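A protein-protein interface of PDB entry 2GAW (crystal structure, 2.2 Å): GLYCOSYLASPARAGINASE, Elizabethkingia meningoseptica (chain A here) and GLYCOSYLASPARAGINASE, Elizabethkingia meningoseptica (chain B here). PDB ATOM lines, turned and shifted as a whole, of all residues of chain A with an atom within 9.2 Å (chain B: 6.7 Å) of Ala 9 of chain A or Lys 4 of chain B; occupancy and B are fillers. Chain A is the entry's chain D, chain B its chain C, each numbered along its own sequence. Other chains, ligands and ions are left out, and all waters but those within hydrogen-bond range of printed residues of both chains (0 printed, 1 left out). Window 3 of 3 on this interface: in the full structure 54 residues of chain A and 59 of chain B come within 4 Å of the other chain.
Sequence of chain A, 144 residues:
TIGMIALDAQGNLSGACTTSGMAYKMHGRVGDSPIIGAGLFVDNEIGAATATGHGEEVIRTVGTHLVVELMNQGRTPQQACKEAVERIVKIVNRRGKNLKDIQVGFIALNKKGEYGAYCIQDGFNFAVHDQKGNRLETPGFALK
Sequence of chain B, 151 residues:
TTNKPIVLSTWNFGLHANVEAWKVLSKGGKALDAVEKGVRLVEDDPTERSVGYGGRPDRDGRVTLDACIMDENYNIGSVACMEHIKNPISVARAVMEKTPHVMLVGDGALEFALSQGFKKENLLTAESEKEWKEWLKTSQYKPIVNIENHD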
ATOM      1  N   ALA A   6     -30.195 -23.768  35.156  1.00  0.00           N
ATOM      2  CA  ALA A   6     -29.744 -23.820  33.771  1.00  0.00           C
ATOM      3  C   ALA A   6     -28.440 -23.092  33.565  1.00  0.00           C
ATOM      4  O   ALA A   6     -28.108 -22.174  34.328  1.00  0.00           O
ATOM      5  CB  ALA A   6     -30.724 -23.167  32.801  1.00  0.00           C
ATOM      6  N   LEU A   7     -27.742 -23.551  32.522  1.00  0.00           N
ATOM      7  CA  LEU A   7     -26.506 -22.978  32.022  1.00  0.00           C
ATOM      8  C   LEU A   7     -26.866 -22.542  30.606  1.00  0.00           C
ATOM      9  O   LEU A   7     -27.328 -23.367  29.800  1.00  0.00           O
ATOM     10  CB  LEU A   7     -25.398 -24.039  31.974  1.00  0.00           C
ATOM     11  CG  LEU A   7     -24.007 -23.666  31.468  1.00  0.00           C
ATOM     12  CD1 LEU A   7     -23.325 -22.747  32.450  1.00  0.00           C
ATOM     13  CD2 LEU A   7     -23.161 -24.924  31.331  1.00  0.00           C
ATOM     14  N   ASP A   8     -26.712 -21.273  30.272  1.00  0.00           N
ATOM     15  CA  ASP A   8     -27.038 -20.798  28.936  1.00  0.00           C
ATOM     16  C   ASP A   8     -25.842 -20.855  27.995  1.00  0.00           C
ATOM     17  O   ASP A   8     -24.748 -21.287  28.359  1.00  0.00           O
ATOM     18  CB  ASP A   8     -27.587 -19.353  28.988  1.00  0.00           C
ATOM     19  CG  ASP A   8     -26.708 -18.293  29.620  1.00  0.00           C
ATOM     20  OD1 ASP A   8     -25.487 -18.371  29.545  1.00  0.00           O
ATOM     21  OD2 ASP A   8     -27.251 -17.371  30.210  1.00  0.00           O
ATOM     22  N   ALA A   9     -26.020 -20.492  26.734  1.00  0.00           N
ATOM     23  CA  ALA A   9     -24.951 -20.514  25.762  1.00  0.00           C
ATOM     24  C   ALA A   9     -23.845 -19.533  26.123  1.00  0.00           C
ATOM     25  O   ALA A   9     -22.689 -19.797  25.748  1.00  0.00           O
ATOM     26  CB  ALA A   9     -25.503 -20.166  24.404  1.00  0.00           C
ATOM     27  N   GLN A  10     -24.114 -18.448  26.867  1.00  0.00           N
ATOM     28  CA  GLN A  10     -23.048 -17.582  27.350  1.00  0.00           C
ATOM     29  C   GLN A  10     -22.236 -18.265  28.437  1.00  0.00           C
ATOM     30  O   GLN A  10     -21.129 -17.801  28.717  1.00  0.00           O
ATOM     31  CB  GLN A  10     -23.549 -16.320  27.967  1.00  0.00           C
ATOM     32  CG  GLN A  10     -24.088 -15.358  26.963  1.00  0.00           C
ATOM     33  CD  GLN A  10     -24.881 -14.277  27.657  1.00  0.00           C
ATOM     34  OE1 GLN A  10     -26.108 -14.345  27.754  1.00  0.00           O
ATOM     35  NE2 GLN A  10     -24.182 -13.252  28.120  1.00  0.00           N
ATOM     36  N   GLY A  11     -22.736 -19.353  29.043  1.00  0.00           N
ATOM     37  CA  GLY A  11     -22.012 -20.069  30.077  1.00  0.00           C
ATOM     38  C   GLY A  11     -22.286 -19.468  31.448  1.00  0.00           C
ATOM     39  O   GLY A  11     -21.431 -19.453  32.344  1.00  0.00           O
ATOM     40  N   ASN A  12     -23.513 -19.027  31.631  1.00  0.00           N
ATOM     41  CA  ASN A  12     -23.974 -18.417  32.849  1.00  0.00           C
ATOM     42  C   ASN A  12     -25.061 -19.281  33.433  1.00  0.00           C
ATOM     43  O   ASN A  12     -25.857 -19.900  32.722  1.00  0.00           O
ATOM     44  CB  ASN A  12     -24.547 -17.047  32.584  1.00  0.00           C
ATOM     45  CG  ASN A  12     -23.509 -15.951  32.418  1.00  0.00           C
ATOM     46  OD1 ASN A  12     -22.324 -16.096  32.729  1.00  0.00           O
ATOM     47  ND2 ASN A  12     -23.908 -14.791  31.946  1.00  0.00           N
ATOM     48  N   LEU A  13     -25.060 -19.356  34.753  1.00  0.00           N
ATOM     49  CA  LEU A  13     -26.014 -20.165  35.485  1.00  0.00           C
ATOM     50  C   LEU A  13     -27.084 -19.279  36.089  1.00  0.00           C
ATOM     51  O   LEU A  13     -26.851 -18.090  36.299  1.00  0.00           O
ATOM     52  CB  LEU A  13     -25.315 -20.928  36.594  1.00  0.00           C
ATOM     53  CG  LEU A  13     -24.327 -22.015  36.226  1.00  0.00           C
ATOM     54  CD1 LEU A  13     -23.377 -22.188  37.373  1.00  0.00           C
ATOM     55  CD2 LEU A  13     -25.058 -23.321  35.896  1.00  0.00           C
ATOM     56  N   LEU A 109     -25.637 -28.877  38.876  1.00  0.00           N
ATOM     57  CA  LEU A 109     -25.071 -28.565  37.584  1.00  0.00           C
ATOM     58  C   LEU A 109     -23.800 -27.778  37.843  1.00  0.00           C
ATOM     59  O   LEU A 109     -23.743 -27.018  38.816  1.00  0.00           O
ATOM     60  CB  LEU A 109     -26.108 -27.753  36.831  1.00  0.00           C
ATOM     61  CG  LEU A 109     -26.023 -27.436  35.361  1.00  0.00           C
ATOM     62  CD1 LEU A 109     -25.974 -28.723  34.546  1.00  0.00           C
ATOM     63  CD2 LEU A 109     -27.234 -26.582  34.995  1.00  0.00           C
ATOM     64  N   ASN A 110     -22.744 -27.968  37.063  1.00  0.00           N
ATOM     65  CA  ASN A 110     -21.569 -27.140  37.235  1.00  0.00           C
ATOM     66  C   ASN A 110     -21.316 -26.335  35.977  1.00  0.00           C
ATOM     67  O   ASN A 110     -22.041 -26.439  34.984  1.00  0.00           O
ATOM     68  CB  ASN A 110     -20.332 -27.986  37.560  1.00  0.00           C
ATOM     69  CG  ASN A 110     -19.740 -28.848  36.458  1.00  0.00           C
ATOM     70  OD1 ASN A 110     -20.105 -28.822  35.281  1.00  0.00           O
ATOM     71  ND2 ASN A 110     -18.760 -29.636  36.830  1.00  0.00           N
ATOM     72  N   LYS A 111     -20.280 -25.506  36.040  1.00  0.00           N
ATOM     73  CA  LYS A 111     -19.884 -24.702  34.898  1.00  0.00           C
ATOM     74  C   LYS A 111     -19.530 -25.399  33.593  1.00  0.00           C
ATOM     75  O   LYS A 111     -19.537 -24.795  32.520  1.00  0.00           O
ATOM     76  CB  LYS A 111     -18.709 -23.804  35.324  1.00  0.00           C
ATOM     77  CG  LYS A 111     -19.327 -22.497  35.780  1.00  0.00           C
ATOM     78  CD  LYS A 111     -20.014 -21.934  34.526  1.00  0.00           C
ATOM     79  CE  LYS A 111     -20.990 -20.867  34.862  1.00  0.00           C
ATOM     80  NZ  LYS A 111     -20.343 -19.596  34.672  1.00  0.00           N
ATOM     81  N   LYS A 112     -19.212 -26.675  33.635  1.00  0.00           N
ATOM     82  CA  LYS A 112     -18.898 -27.393  32.429  1.00  0.00           C
ATOM     83  C   LYS A 112     -20.148 -27.943  31.756  1.00  0.00           C
ATOM     84  O   LYS A 112     -20.052 -28.396  30.620  1.00  0.00           O
ATOM     85  CB  LYS A 112     -17.943 -28.516  32.787  1.00  0.00           C
ATOM     86  CG  LYS A 112     -16.544 -28.133  33.212  1.00  0.00           C
ATOM     87  CD  LYS A 112     -15.625 -28.212  32.007  1.00  0.00           C
ATOM     88  CE  LYS A 112     -15.630 -26.920  31.167  1.00  0.00           C
ATOM     89  NZ  LYS A 112     -15.174 -27.169  29.813  1.00  0.00           N
ATOM     90  N   GLY A 113     -21.322 -27.884  32.376  1.00  0.00           N
ATOM     91  CA  GLY A 113     -22.511 -28.511  31.825  1.00  0.00           C
ATOM     92  C   GLY A 113     -22.634 -29.950  32.332  1.00  0.00           C
ATOM     93  O   GLY A 113     -23.476 -30.729  31.864  1.00  0.00           O
ATOM     94  N   GLU A 114     -21.773 -30.370  33.282  1.00  0.00           N
ATOM     95  CA  GLU A 114     -21.896 -31.671  33.930  1.00  0.00           C
ATOM     96  C   GLU A 114     -23.037 -31.520  34.925  1.00  0.00           C
ATOM     97  O   GLU A 114     -23.231 -30.441  35.504  1.00  0.00           O
ATOM     98  CB  GLU A 114     -20.634 -32.048  34.692  1.00  0.00           C
ATOM     99  CG  GLU A 114     -19.436 -32.170  33.771  1.00  0.00           C
ATOM    100  CD  GLU A 114     -18.072 -32.330  34.433  1.00  0.00           C
ATOM    101  OE1 GLU A 114     -17.849 -31.984  35.587  1.00  0.00           O
ATOM    102  OE2 GLU A 114     -17.156 -32.768  33.762  1.00  0.00           O
ATOM    103  N   HIS A 129     -32.470 -31.339  29.799  1.00  0.00           N
ATOM    104  CA  HIS A 129     -32.596 -30.983  28.401  1.00  0.00           C
ATOM    105  C   HIS A 129     -31.341 -30.250  27.987  1.00  0.00           C
ATOM    106  O   HIS A 129     -31.113 -29.116  28.423  1.00  0.00           O
ATOM    107  CB  HIS A 129     -33.764 -30.055  28.126  1.00  0.00           C
ATOM    108  CG  HIS A 129     -34.117 -29.963  26.642  1.00  0.00           C
ATOM    109  ND1 HIS A 129     -33.371 -30.175  25.553  1.00  0.00           N
ATOM    110  CD2 HIS A 129     -35.382 -29.635  26.208  1.00  0.00           C
ATOM    111  CE1 HIS A 129     -34.130 -29.996  24.499  1.00  0.00           C
ATOM    112  NE2 HIS A 129     -35.333 -29.673  24.905  1.00  0.00           N
ATOM    113  N   ASP A 130     -30.538 -30.914  27.175  1.00  0.00           N
ATOM    114  CA  ASP A 130     -29.369 -30.302  26.587  1.00  0.00           C
ATOM    115  C   ASP A 130     -29.558 -30.431  25.079  1.00  0.00           C
ATOM    116  O   ASP A 130     -30.706 -30.586  24.605  1.00  0.00           O
ATOM    117  CB  ASP A 130     -28.082 -31.015  27.071  1.00  0.00           C
ATOM    118  CG  ASP A 130     -27.933 -32.515  26.892  1.00  0.00           C
ATOM    119  OD1 ASP A 130     -28.567 -33.136  26.050  1.00  0.00           O
ATOM    120  OD2 ASP A 130     -27.142 -33.128  27.607  1.00  0.00           O
ATOM    121  N   GLN A 131     -28.473 -30.223  24.327  1.00  0.00           N
ATOM    122  CA  GLN A 131     -28.508 -30.259  22.876  1.00  0.00           C
ATOM    123  C   GLN A 131     -28.747 -31.650  22.324  1.00  0.00           C
ATOM    124  O   GLN A 131     -29.063 -31.777  21.150  1.00  0.00           O
ATOM    125  CB  GLN A 131     -27.195 -29.711  22.312  1.00  0.00           C
ATOM    126  CG  GLN A 131     -27.115 -28.189  22.363  1.00  0.00           C
ATOM    127  CD  GLN A 131     -25.835 -27.570  21.782  1.00  0.00           C
ATOM    128  OE1 GLN A 131     -25.165 -28.088  20.881  1.00  0.00           O
ATOM    129  NE2 GLN A 131     -25.465 -26.390  22.253  1.00  0.00           N
ATOM    130  N   LYS A 132     -28.583 -32.706  23.123  1.00  0.00           N
ATOM    131  CA  LYS A 132     -28.832 -34.057  22.651  1.00  0.00           C
ATOM    132  C   LYS A 132     -30.306 -34.386  22.823  1.00  0.00           C
ATOM    133  O   LYS A 132     -30.761 -35.421  22.327  1.00  0.00           O
ATOM    134  CB  LYS A 132     -27.997 -35.056  23.438  1.00  0.00           C
ATOM    135  CG  LYS A 132     -26.494 -34.829  23.349  1.00  0.00           C
ATOM    136  CD  LYS A 132     -25.709 -35.925  24.087  1.00  0.00           C
ATOM    137  CE  LYS A 132     -26.070 -36.069  25.572  1.00  0.00           C
ATOM    138  NZ  LYS A 132     -25.850 -34.830  26.285  1.00  0.00           N
ATOM    139  N   ASN B   3     -20.844 -28.554  27.636  1.00  0.00           N
ATOM    140  CA  ASN B   3     -22.204 -29.015  27.384  1.00  0.00           C
ATOM    141  C   ASN B   3     -23.207 -27.921  27.732  1.00  0.00           C
ATOM    142  O   ASN B   3     -23.749 -27.888  28.833  1.00  0.00           O
ATOM    143  CB  ASN B   3     -22.505 -30.262  28.215  1.00  0.00           C
ATOM    144  CG  ASN B   3     -23.809 -30.937  27.801  1.00  0.00           C
ATOM    145  OD1 ASN B   3     -24.260 -30.794  26.662  1.00  0.00           O
ATOM    146  ND2 ASN B   3     -24.461 -31.746  28.630  1.00  0.00           N
ATOM    147  N   LYS B   4     -23.378 -26.933  26.859  1.00  0.00           N
ATOM    148  CA  LYS B   4     -24.309 -25.853  27.140  1.00  0.00           C
ATOM    149  C   LYS B   4     -25.061 -25.520  25.856  1.00  0.00           C
ATOM    150  O   LYS B   4     -24.507 -25.777  24.781  1.00  0.00           O
ATOM    151  CB  LYS B   4     -23.564 -24.610  27.660  1.00  0.00           C
ATOM    152  CG  LYS B   4     -22.467 -24.002  26.786  1.00  0.00           C
ATOM    153  CD  LYS B   4     -21.751 -22.928  27.594  1.00  0.00           C
ATOM    154  CE  LYS B   4     -20.508 -22.416  26.864  1.00  0.00           C
ATOM    155  NZ  LYS B   4     -20.847 -21.565  25.740  1.00  0.00           N
ATOM    156  N   PRO B   5     -26.293 -24.992  25.855  1.00  0.00           N
ATOM    157  CA  PRO B   5     -27.139 -24.841  27.033  1.00  0.00           C
ATOM    158  C   PRO B   5     -27.623 -26.174  27.591  1.00  0.00           C
ATOM    159  O   PRO B   5     -27.583 -27.189  26.892  1.00  0.00           O
ATOM    160  CB  PRO B   5     -28.277 -23.964  26.572  1.00  0.00           C
ATOM    161  CG  PRO B   5     -27.824 -23.348  25.284  1.00  0.00           C
ATOM    162  CD  PRO B   5     -26.961 -24.443  24.681  1.00  0.00           C
ATOM    163  N   ILE B   6     -28.035 -26.191  28.851  1.00  0.00           N
ATOM    164  CA  ILE B   6     -28.591 -27.377  29.480  1.00  0.00           C
ATOM    165  C   ILE B   6     -29.461 -26.903  30.646  1.00  0.00           C
ATOM    166  O   ILE B   6     -29.093 -25.935  31.328  1.00  0.00           O
ATOM    167  CB  ILE B   6     -27.422 -28.341  29.940  1.00  0.00           C
ATOM    168  CG1 ILE B   6     -28.041 -29.586  30.573  1.00  0.00           C
ATOM    169  CG2 ILE B   6     -26.445 -27.637  30.869  1.00  0.00           C
ATOM    170  CD1 ILE B   6     -27.010 -30.676  30.884  1.00  0.00           C
ATOM    171  N   TRP B  22     -36.210 -24.355  27.193  1.00  0.00           N
ATOM    172  CA  TRP B  22     -35.369 -24.595  26.035  1.00  0.00           C
ATOM    173  C   TRP B  22     -35.722 -23.664  24.896  1.00  0.00           C
ATOM    174  O   TRP B  22     -34.848 -23.352  24.088  1.00  0.00           O
ATOM    175  CB  TRP B  22     -35.503 -26.024  25.536  1.00  0.00           C
ATOM    176  CG  TRP B  22     -34.356 -26.424  24.613  1.00  0.00           C
ATOM    177  CD1 TRP B  22     -34.561 -26.683  23.275  1.00  0.00           C
ATOM    178  CD2 TRP B  22     -33.044 -26.583  24.988  1.00  0.00           C
ATOM    179  NE1 TRP B  22     -33.383 -27.011  22.799  1.00  0.00           N
ATOM    180  CE2 TRP B  22     -32.451 -26.964  23.772  1.00  0.00           C
ATOM    181  CE3 TRP B  22     -32.277 -26.464  26.154  1.00  0.00           C
ATOM    182  CZ2 TRP B  22     -31.084 -27.235  23.698  1.00  0.00           C
ATOM    183  CZ3 TRP B  22     -30.913 -26.739  26.080  1.00  0.00           C
ATOM    184  CH2 TRP B  22     -30.323 -27.114  24.863  1.00  0.00           C
ATOM    185  N   LEU B  25     -33.338 -20.962  25.775  1.00  0.00           N
ATOM    186  CA  LEU B  25     -31.962 -21.408  25.706  1.00  0.00           C
ATOM    187  C   LEU B  25     -31.442 -21.756  24.322  1.00  0.00           C
ATOM    188  O   LEU B  25     -30.319 -21.358  23.987  1.00  0.00           O
ATOM    189  CB  LEU B  25     -31.769 -22.608  26.616  1.00  0.00           C
ATOM    190  CG  LEU B  25     -31.863 -22.399  28.129  1.00  0.00           C
ATOM    191  CD1 LEU B  25     -31.567 -23.713  28.818  1.00  0.00           C
ATOM    192  CD2 LEU B  25     -30.859 -21.355  28.600  1.00  0.00           C
ATOM    193  N   LYS B  27     -32.207 -20.466  21.554  1.00  0.00           N
ATOM    194  CA  LYS B  27     -32.035 -19.267  20.753  1.00  0.00           C
ATOM    195  C   LYS B  27     -30.913 -18.386  21.286  1.00  0.00           C
ATOM    196  O   LYS B  27     -30.752 -17.248  20.847  1.00  0.00           O
ATOM    197  CB  LYS B  27     -33.358 -18.496  20.725  1.00  0.00           C
ATOM    198  CG  LYS B  27     -34.444 -19.340  20.095  1.00  0.00           C
ATOM    199  CD  LYS B  27     -35.706 -18.516  19.859  1.00  0.00           C
ATOM    200  CE  LYS B  27     -36.906 -19.410  19.544  1.00  0.00           C
ATOM    201  NZ  LYS B  27     -37.329 -20.122  20.732  1.00  0.00           N
ATOM    202  N   GLY B  28     -30.111 -18.905  22.226  1.00  0.00           N
ATOM    203  CA  GLY B  28     -29.017 -18.169  22.842  1.00  0.00           C
ATOM    204  C   GLY B  28     -29.491 -17.109  23.839  1.00  0.00           C
ATOM    205  O   GLY B  28     -28.848 -16.049  23.990  1.00  0.00           O
ATOM    206  N   GLY B  29     -30.651 -17.416  24.441  1.00  0.00           N
ATOM    207  CA  GLY B  29     -31.284 -16.582  25.447  1.00  0.00           C
ATOM    208  C   GLY B  29     -30.625 -16.767  26.814  1.00  0.00           C
ATOM    209  O   GLY B  29     -29.878 -17.723  27.037  1.00  0.00           O
ATOM    210  N   ALA B  31     -30.148 -17.615  30.720  1.00  0.00           N
ATOM    211  CA  ALA B  31     -30.555 -18.672  31.638  1.00  0.00           C
ATOM    212  C   ALA B  31     -31.632 -18.156  32.567  1.00  0.00           C
ATOM    213  O   ALA B  31     -32.624 -18.847  32.792  1.00  0.00           O
ATOM    214  CB  ALA B  31     -29.390 -19.134  32.490  1.00  0.00           C
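The backbone NH (N) of Asn 12 of chain A lies within hydrogen-bond range of the side-chain carboxylate (OD1) of Asp 8 of chain A, 2.9 Å away.
The side-chain amino group (NZ) of Lys 111 of chain A sits at hydrogen-bond distance from the backbone carbonyl oxygen (O) of Gly 11 of chain A (2.6 Å).
The backbone NH (N) of Gly 11 of chain A lies within hydrogen-bond range of the side-chain carboxylate (OD1) of Asp 8 of chain A (3.0 Å).
The side-chain amide oxygen of Asn 110 of chain A is in hydrogen-bond range of the backbone NH of Gly 113 of chain A (3.3 Å).
The side-chain amide oxygen (OD1) of Asn 110 of chain A is in hydrogen-bond range of the backbone NH (N) of Lys 112 of chain A, 2.8 Å away.
The side-chain carboxylate of Asp 8 of chain A lies within hydrogen-bond range of the backbone NH of Gln 10 of chain A, at 3.0 Å.
Asp 8 of chain A touches Lys 4 of chain B.
Asp 8 of chain A touches Leu 25 of chain B.
CA of Gly 11 of chain A touches CD of Lys 4 of chain B (3.8 Å).
Ala 31 of chain B touches Asn 12 of chain A (CB to O, 3.6 Å).
CD1 of Leu 109 of chain A touches CG2 of Ile 6 of chain B, 3.9 Å away.
Gly 113 of chain A touches Ile 6 of chain B (O to CD1, 3.7 Å).
Ile 6 of chain B touches His 129 of chain A (CA to O, 3.2 Å).
Trp 22 of chain B touches His 129 of chain A (CZ3 to O, 3.3 Å).
CA of Asp 130 of chain A touches O of Pro 5 of chain B (3.6 Å).
Asp 130 of chain A touches Ile 6 of chain B.
Of the 10 printed residues of chain B, 8 touch a printed residue of chain A.
Printed residues of chain A that touch a printed residue of chain B: Ala 6, Leu 7, Asp 8, Ala 9, Gly 11, Asn 12, Leu 109, Lys 112, Gly 113, His 129, Asp 130 and Gln 131.
Hydrophobic or aromatic side chains of chain A within 4 Å of the printed part of chain B: Ala 6, Leu 7, Leu 109 and His 129.
Among the printed residues, 27 pairs touch across the chains.
Of chain B, only Lys 4 and Pro 5 come within 4 Å of Ala 9 of chain A.
Of the printed residues of chain A, Lys 4 of chain B touches Leu 7, Asp 8, Ala 9, Gly 11 and Gln 131.
Of the printed residues of chain A, Ile 6 of chain B touches Ala 6 (3.3 Å), Leu 7 (3.0 Å), Leu 109 (3.9 Å), Gly 113 (3.7 Å), His 129 (3.2 Å) and Asp 130 (3.8 Å).
Printed residues of chain B within 4 Å of Asp 8 of chain A: Lys 4 (3.5 Å), Leu 25 (3.9 Å), Gly 29 (3.4 Å) and Ala 31 (3.0 Å).
Printed residues of chain B within 4 Å of Gly 113 of chain A: Asn 3 (3.3 Å) and Ile 6 (3.7 Å).
Printed residues of chain B within 4 Å of Asn 12 of chain A: Ala 31 (3.6 Å).
The nearest residue of chain B that does not touch Ala 9 of chain A is Gly 28 of chain B (4.3 Å).
The backbone carbonyl oxygen (O) of Ala 9 of chain A sits at hydrogen-bond distance from the side-chain amino group (NZ) of Lys 4 of chain B (2.6 Å).
The side-chain amide nitrogen of Asn 3 of chain B sits at hydrogen-bond distance from the side-chain carboxylate of Asp 130 of chain A, at 3.2 Å.
NE2 of Gln 131 of chain A lies within hydrogen-bond range of O of Lys 4 of chain B.
The backbone NH (N) of Asn 3 of chain B is in hydrogen-bond range of the backbone carbonyl oxygen (O) of Lys 112 of chain A (3.1 Å).
N of Ala 31 of chain B sits at hydrogen-bond distance from OD2 of Asp 8 of chain A (3.0 Å).
The backbone NH (N) of Leu 7 of chain A sits at hydrogen-bond distance from the backbone carbonyl oxygen (O) of Ile 6 of chain B, 3.0 Å away.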
